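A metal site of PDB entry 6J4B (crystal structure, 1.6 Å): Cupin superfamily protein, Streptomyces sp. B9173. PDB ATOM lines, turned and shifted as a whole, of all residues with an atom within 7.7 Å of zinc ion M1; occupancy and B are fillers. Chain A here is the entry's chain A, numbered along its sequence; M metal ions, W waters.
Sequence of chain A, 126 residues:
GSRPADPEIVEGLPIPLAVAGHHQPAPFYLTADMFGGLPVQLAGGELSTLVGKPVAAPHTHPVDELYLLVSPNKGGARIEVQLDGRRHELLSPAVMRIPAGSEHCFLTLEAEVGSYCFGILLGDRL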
ATOM      1  N   VAL A  19      16.920 -20.447 -17.208  1.00  0.00           N
ATOM      2  CA  VAL A  19      17.432 -19.978 -18.503  1.00  0.00           C
ATOM      3  C   VAL A  19      16.586 -18.779 -18.980  1.00  0.00           C
ATOM      4  O   VAL A  19      15.353 -18.827 -18.879  1.00  0.00           O
ATOM      5  CB  VAL A  19      17.362 -21.111 -19.583  1.00  0.00           C
ATOM      6  CG1 VAL A  19      17.817 -20.648 -20.932  1.00  0.00           C
ATOM      7  CG2 VAL A  19      18.256 -22.298 -19.149  1.00  0.00           C
ATOM      8  N   HIS A  22      12.665 -18.392 -20.440  1.00  0.00           N
ATOM      9  CA  HIS A  22      11.806 -19.478 -19.977  1.00  0.00           C
ATOM     10  C   HIS A  22      10.950 -19.094 -18.800  1.00  0.00           C
ATOM     11  O   HIS A  22      11.204 -18.051 -18.179  1.00  0.00           O
ATOM     12  CB  HIS A  22      12.712 -20.701 -19.602  1.00  0.00           C
ATOM     13  CG  HIS A  22      13.440 -21.311 -20.790  1.00  0.00           C
ATOM     14  ND1 HIS A  22      14.336 -20.637 -21.572  1.00  0.00           N
ATOM     15  CD2 HIS A  22      13.351 -22.556 -21.298  1.00  0.00           C
ATOM     16  CE1 HIS A  22      14.821 -21.452 -22.494  1.00  0.00           C
ATOM     17  NE2 HIS A  22      14.233 -22.627 -22.332  1.00  0.00           N
ATOM     18  N   HIS A  59      15.385 -16.327 -27.077  1.00  0.00           N
ATOM     19  CA  HIS A  59      16.520 -16.238 -26.218  1.00  0.00           C
ATOM     20  C   HIS A  59      17.759 -16.579 -27.010  1.00  0.00           C
ATOM     21  O   HIS A  59      17.684 -16.987 -28.164  1.00  0.00           O
ATOM     22  CB  HIS A  59      16.351 -17.143 -24.965  1.00  0.00           C
ATOM     23  CG  HIS A  59      16.058 -18.597 -25.306  1.00  0.00           C
ATOM     24  ND1 HIS A  59      14.820 -18.959 -25.774  1.00  0.00           N
ATOM     25  CD2 HIS A  59      16.813 -19.716 -25.302  1.00  0.00           C
ATOM     26  CE1 HIS A  59      14.816 -20.255 -26.064  1.00  0.00           C
ATOM     27  NE2 HIS A  59      16.015 -20.731 -25.763  1.00  0.00           N
ATOM     28  N   THR A  60      18.889 -16.257 -26.397  1.00  0.00           N
ATOM     29  CA  THR A  60      20.239 -16.477 -27.020  1.00  0.00           C
ATOM     30  C   THR A  60      21.189 -17.263 -26.124  1.00  0.00           C
ATOM     31  O   THR A  60      20.991 -17.310 -24.931  1.00  0.00           O
ATOM     32  CB  THR A  60      20.948 -15.127 -27.366  1.00  0.00           C
ATOM     33  OG1 THR A  60      21.314 -14.445 -26.140  1.00  0.00           O
ATOM     34  CG2 THR A  60      20.075 -14.210 -28.226  1.00  0.00           C
ATOM     35  N   HIS A  61      22.205 -17.889 -26.738  1.00  0.00           N
ATOM     36  CA  HIS A  61      23.345 -18.417 -26.050  1.00  0.00           C
ATOM     37  C   HIS A  61      24.632 -17.768 -26.677  1.00  0.00           C
ATOM     38  O   HIS A  61      24.643 -17.405 -27.854  1.00  0.00           O
ATOM     39  CB  HIS A  61      23.457 -19.941 -26.250  1.00  0.00           C
ATOM     40  CG  HIS A  61      22.136 -20.672 -26.177  1.00  0.00           C
ATOM     41  ND1 HIS A  61      21.392 -20.762 -25.018  1.00  0.00           N
ATOM     42  CD2 HIS A  61      21.428 -21.314 -27.129  1.00  0.00           C
ATOM     43  CE1 HIS A  61      20.287 -21.474 -25.280  1.00  0.00           C
ATOM     44  NE2 HIS A  61      20.291 -21.800 -26.567  1.00  0.00           N
ATOM     45  N   VAL A  63      27.214 -19.479 -27.412  1.00  0.00           N
ATOM     46  CA  VAL A  63      27.848 -20.528 -28.203  1.00  0.00           C
ATOM     47  C   VAL A  63      26.879 -21.041 -29.237  1.00  0.00           C
ATOM     48  O   VAL A  63      25.671 -20.880 -29.047  1.00  0.00           O
ATOM     49  CB  VAL A  63      28.387 -21.677 -27.307  1.00  0.00           C
ATOM     50  CG1 VAL A  63      29.378 -21.122 -26.257  1.00  0.00           C
ATOM     51  CG2 VAL A  63      27.256 -22.350 -26.544  1.00  0.00           C
ATOM     52  N   ASP A  64      27.376 -21.644 -30.332  1.00  0.00           N
ATOM     53  CA  ASP A  64      26.528 -22.312 -31.289  1.00  0.00           C
ATOM     54  C   ASP A  64      25.783 -23.488 -30.581  1.00  0.00           C
ATOM     55  O   ASP A  64      26.281 -24.076 -29.615  1.00  0.00           O
ATOM     56  CB  ASP A  64      27.292 -22.895 -32.471  1.00  0.00           C
ATOM     57  CG  ASP A  64      27.872 -21.874 -33.369  1.00  0.00           C
ATOM     58  OD1 ASP A  64      27.472 -20.675 -33.319  1.00  0.00           O
ATOM     59  OD2 ASP A  64      28.764 -22.303 -34.156  1.00  0.00           O
ATOM     60  N   GLU A  65      24.652 -23.832 -31.153  1.00  0.00           N
ATOM     61  CA  GLU A  65      23.802 -24.945 -30.552  1.00  0.00           C
ATOM     62  C   GLU A  65      23.262 -25.708 -31.756  1.00  0.00           C
ATOM     63  O   GLU A  65      23.011 -25.148 -32.833  1.00  0.00           O
ATOM     64  CB  GLU A  65      22.633 -24.413 -29.783  1.00  0.00           C
ATOM     65  CG  GLU A  65      21.651 -25.405 -29.174  1.00  0.00           C
ATOM     66  CD  GLU A  65      20.587 -24.686 -28.464  1.00  0.00           C
ATOM     67  OE1 GLU A  65      20.036 -23.673 -28.986  1.00  0.00           O
ATOM     68  OE2 GLU A  65      20.244 -25.131 -27.396  1.00  0.00           O
ATOM     69  N   LEU A  66      23.096 -27.002 -31.566  1.00  0.00           N
ATOM     70  CA  LEU A  66      22.473 -27.856 -32.542  1.00  0.00           C
ATOM     71  C   LEU A  66      21.192 -28.489 -31.988  1.00  0.00           C
ATOM     72  O   LEU A  66      21.237 -29.092 -30.888  1.00  0.00           O
ATOM     73  CB  LEU A  66      23.398 -29.015 -32.999  1.00  0.00           C
ATOM     74  CG  LEU A  66      24.802 -28.581 -33.417  1.00  0.00           C
ATOM     75  CD1 LEU A  66      25.764 -29.688 -33.720  1.00  0.00           C
ATOM     76  CD2 LEU A  66      24.692 -27.641 -34.602  1.00  0.00           C
ATOM     77  N   TYR A  67      20.077 -28.270 -32.663  1.00  0.00           N
ATOM     78  CA  TYR A  67      18.805 -28.940 -32.297  1.00  0.00           C
ATOM     79  C   TYR A  67      18.793 -30.296 -32.955  1.00  0.00           C
ATOM     80  O   TYR A  67      19.102 -30.415 -34.142  1.00  0.00           O
ATOM     81  CB  TYR A  67      17.603 -28.106 -32.741  1.00  0.00           C
ATOM     82  CG  TYR A  67      17.137 -27.065 -31.820  1.00  0.00           C
ATOM     83  CD1 TYR A  67      17.910 -26.618 -30.795  1.00  0.00           C
ATOM     84  CD2 TYR A  67      16.004 -26.401 -32.067  1.00  0.00           C
ATOM     85  CE1 TYR A  67      17.419 -25.649 -29.870  1.00  0.00           C
ATOM     86  CE2 TYR A  67      15.504 -25.431 -31.184  1.00  0.00           C
ATOM     87  CZ  TYR A  67      16.212 -25.087 -30.082  1.00  0.00           C
ATOM     88  OH  TYR A  67      15.667 -24.112 -29.206  1.00  0.00           O
ATOM     89  N   ILE A  98      21.789 -23.554 -34.735  1.00  0.00           N
ATOM     90  CA  ILE A  98      21.367 -22.298 -34.107  1.00  0.00           C
ATOM     91  C   ILE A  98      22.647 -21.489 -33.802  1.00  0.00           C
ATOM     92  O   ILE A  98      23.378 -21.757 -32.855  1.00  0.00           O
ATOM     93  CB  ILE A  98      20.605 -22.566 -32.801  1.00  0.00           C
ATOM     94  CG1 ILE A  98      19.471 -23.615 -32.934  1.00  0.00           C
ATOM     95  CG2 ILE A  98      20.080 -21.227 -32.230  1.00  0.00           C
ATOM     96  CD1 ILE A  98      18.410 -23.192 -33.903  1.00  0.00           C
ATOM     97  N   SER A 102      22.048 -15.834 -31.999  1.00  0.00           N
ATOM     98  CA  SER A 102      20.830 -15.824 -32.689  1.00  0.00           C
ATOM     99  C   SER A 102      19.680 -15.876 -31.712  1.00  0.00           C
ATOM    100  O   SER A 102      19.684 -16.749 -30.779  1.00  0.00           O
ATOM    101  CB  SER A 102      20.724 -17.020 -33.609  1.00  0.00           C
ATOM    102  OG  SER A 102      19.469 -17.047 -34.235  1.00  0.00           O
ATOM    103  N   HIS A 104      16.233 -17.105 -30.699  1.00  0.00           N
ATOM    104  CA  HIS A 104      15.550 -18.276 -31.187  1.00  0.00           C
ATOM    105  C   HIS A 104      14.705 -18.899 -30.104  1.00  0.00           C
ATOM    106  O   HIS A 104      14.805 -18.584 -28.900  1.00  0.00           O
ATOM    107  CB  HIS A 104      16.554 -19.344 -31.695  1.00  0.00           C
ATOM    108  CG  HIS A 104      17.398 -19.897 -30.580  1.00  0.00           C
ATOM    109  ND1 HIS A 104      18.461 -19.230 -30.007  1.00  0.00           N
ATOM    110  CD2 HIS A 104      17.270 -21.050 -29.877  1.00  0.00           C
ATOM    111  CE1 HIS A 104      18.982 -19.974 -29.049  1.00  0.00           C
ATOM    112  NE2 HIS A 104      18.237 -21.063 -28.940  1.00  0.00           N
ATOM    113  N   CYS A 105      13.811 -19.767 -30.589  1.00  0.00           N
ATOM    114  CA  CYS A 105      12.894 -20.521 -29.718  1.00  0.00           C
ATOM    115  C   CYS A 105      12.188 -21.542 -30.578  1.00  0.00           C
ATOM    116  O   CYS A 105      12.264 -21.439 -31.802  1.00  0.00           O
ATOM    117  CB  CYS A 105      11.925 -19.644 -28.998  1.00  0.00           C
ATOM    118  SG  CYS A 105      10.993 -18.572 -30.041  1.00  0.00           S
ATOM    119  N   PHE A 106      11.516 -22.467 -29.934  1.00  0.00           N
ATOM    120  CA  PHE A 106      10.779 -23.503 -30.704  1.00  0.00           C
ATOM    121  C   PHE A 106       9.363 -23.689 -30.173  1.00  0.00           C
ATOM    122  O   PHE A 106       9.053 -23.409 -28.986  1.00  0.00           O
ATOM    123  CB  PHE A 106      11.488 -24.862 -30.838  1.00  0.00           C
ATOM    124  CG  PHE A 106      11.327 -25.781 -29.662  1.00  0.00           C
ATOM    125  CD1 PHE A 106      12.108 -25.654 -28.494  1.00  0.00           C
ATOM    126  CD2 PHE A 106      10.436 -26.837 -29.679  1.00  0.00           C
ATOM    127  CE1 PHE A 106      11.888 -26.497 -27.405  1.00  0.00           C
ATOM    128  CE2 PHE A 106      10.266 -27.693 -28.653  1.00  0.00           C
ATOM    129  CZ  PHE A 106      10.991 -27.557 -27.473  1.00  0.00           C
ATOM    130  N   GLY A 119      18.826 -29.765 -27.364  1.00  0.00           N
ATOM    131  CA  GLY A 119      19.749 -28.746 -27.834  1.00  0.00           C
ATOM    132  C   GLY A 119      21.128 -29.026 -27.316  1.00  0.00           C
ATOM    133  O   GLY A 119      21.329 -29.184 -26.058  1.00  0.00           O
ATOM    134  N   ILE A 120      22.056 -29.288 -28.210  1.00  0.00           N
ATOM    135  CA  ILE A 120      23.458 -29.559 -27.908  1.00  0.00           C
ATOM    136  C   ILE A 120      24.221 -28.262 -28.031  1.00  0.00           C
ATOM    137  O   ILE A 120      24.399 -27.748 -29.117  1.00  0.00           O
ATOM    138  CB  ILE A 120      24.058 -30.692 -28.766  1.00  0.00           C
ATOM    139  CG1 ILE A 120      23.291 -32.075 -28.659  1.00  0.00           C
ATOM    140  CG2 ILE A 120      25.507 -30.889 -28.423  1.00  0.00           C
ATOM    141  CD1 ILE A 120      22.156 -32.264 -29.625  1.00  0.00           C
ATOM    142  N   LEU A 121      24.666 -27.742 -26.879  1.00  0.00           N
ATOM    143  CA  LEU A 121      25.362 -26.449 -26.794  1.00  0.00           C
ATOM    144  C   LEU A 121      26.883 -26.690 -26.944  1.00  0.00           C
ATOM    145  O   LEU A 121      27.487 -27.460 -26.143  1.00  0.00           O
ATOM    146  CB  LEU A 121      25.082 -25.759 -25.480  1.00  0.00           C
ATOM    147  CG  LEU A 121      23.638 -25.350 -25.269  1.00  0.00           C
ATOM    148  CD1 LEU A 121      23.242 -25.480 -23.793  1.00  0.00           C
ATOM    149  CD2 LEU A 121      23.378 -23.980 -25.867  1.00  0.00           C
ATOM    150  N   LEU A 126      26.449 -20.583 -20.751  1.00  0.00           N
ATOM    151  CA  LEU A 126      25.140 -20.141 -21.143  1.00  0.00           C
ATOM    152  C   LEU A 126      25.055 -18.622 -21.211  1.00  0.00           C
ATOM    153  O   LEU A 126      24.026 -18.156 -21.689  1.00  0.00           O
ATOM    154  CB  LEU A 126      24.085 -20.614 -20.126  1.00  0.00           C
ATOM    155  CG  LEU A 126      23.812 -22.118 -20.117  1.00  0.00           C
ATOM    156  CD1 LEU A 126      22.885 -22.472 -18.935  1.00  0.00           C
ATOM    157  CD2 LEU A 126      23.212 -22.479 -21.463  1.00  0.00           C
ATOM    158  OXT LEU A 126      25.993 -17.904 -20.744  1.00  0.00           O
HETATM  159 ZN    ZN M   1      18.905 -22.686 -27.787  1.00  0.00          ZN
HETATM  160 ZN    ZN M   2      16.341 -22.728 -25.676  1.00  0.00          ZN
HETATM  161 ZN    ZN M   3      14.688 -24.278 -23.433  1.00  0.00          ZN
HETATM  162  O   HOH W   1      17.276 -23.564 -27.129  1.00  0.00           O
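The backbone NH (N) of His 104 sits at hydrogen-bond distance from the backbone carbonyl oxygen (O) of His 59, at 2.9 Å. The backbone NH of Ile 98 is in hydrogen-bond range of the backbone carbonyl oxygen of Glu 65, 2.8 Å away. A ring nitrogen (ND1) of His 104 is in hydrogen-bond range of the backbone carbonyl oxygen of Ser 102 (2.9 Å).
Residues that only touch zinc ion M1: Tyr 67 (3.8 Å). The nearest printed residue that does not touch zinc ion M1 is His 59 (4.03 Å).
Zinc ion M1 is bound by the side-chain carboxylate of Glu 65, water W1, a ring nitrogen (NE2) of His 61 and a ring nitrogen (NE2) of His 104. Slightly farther from zinc ion M1 lies OE2 of Glu 65 (2.8 Å).
Water W1 bridges OH of Tyr 67 (2.7 Å) and OE2 of Glu 65 (3.4 Å).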
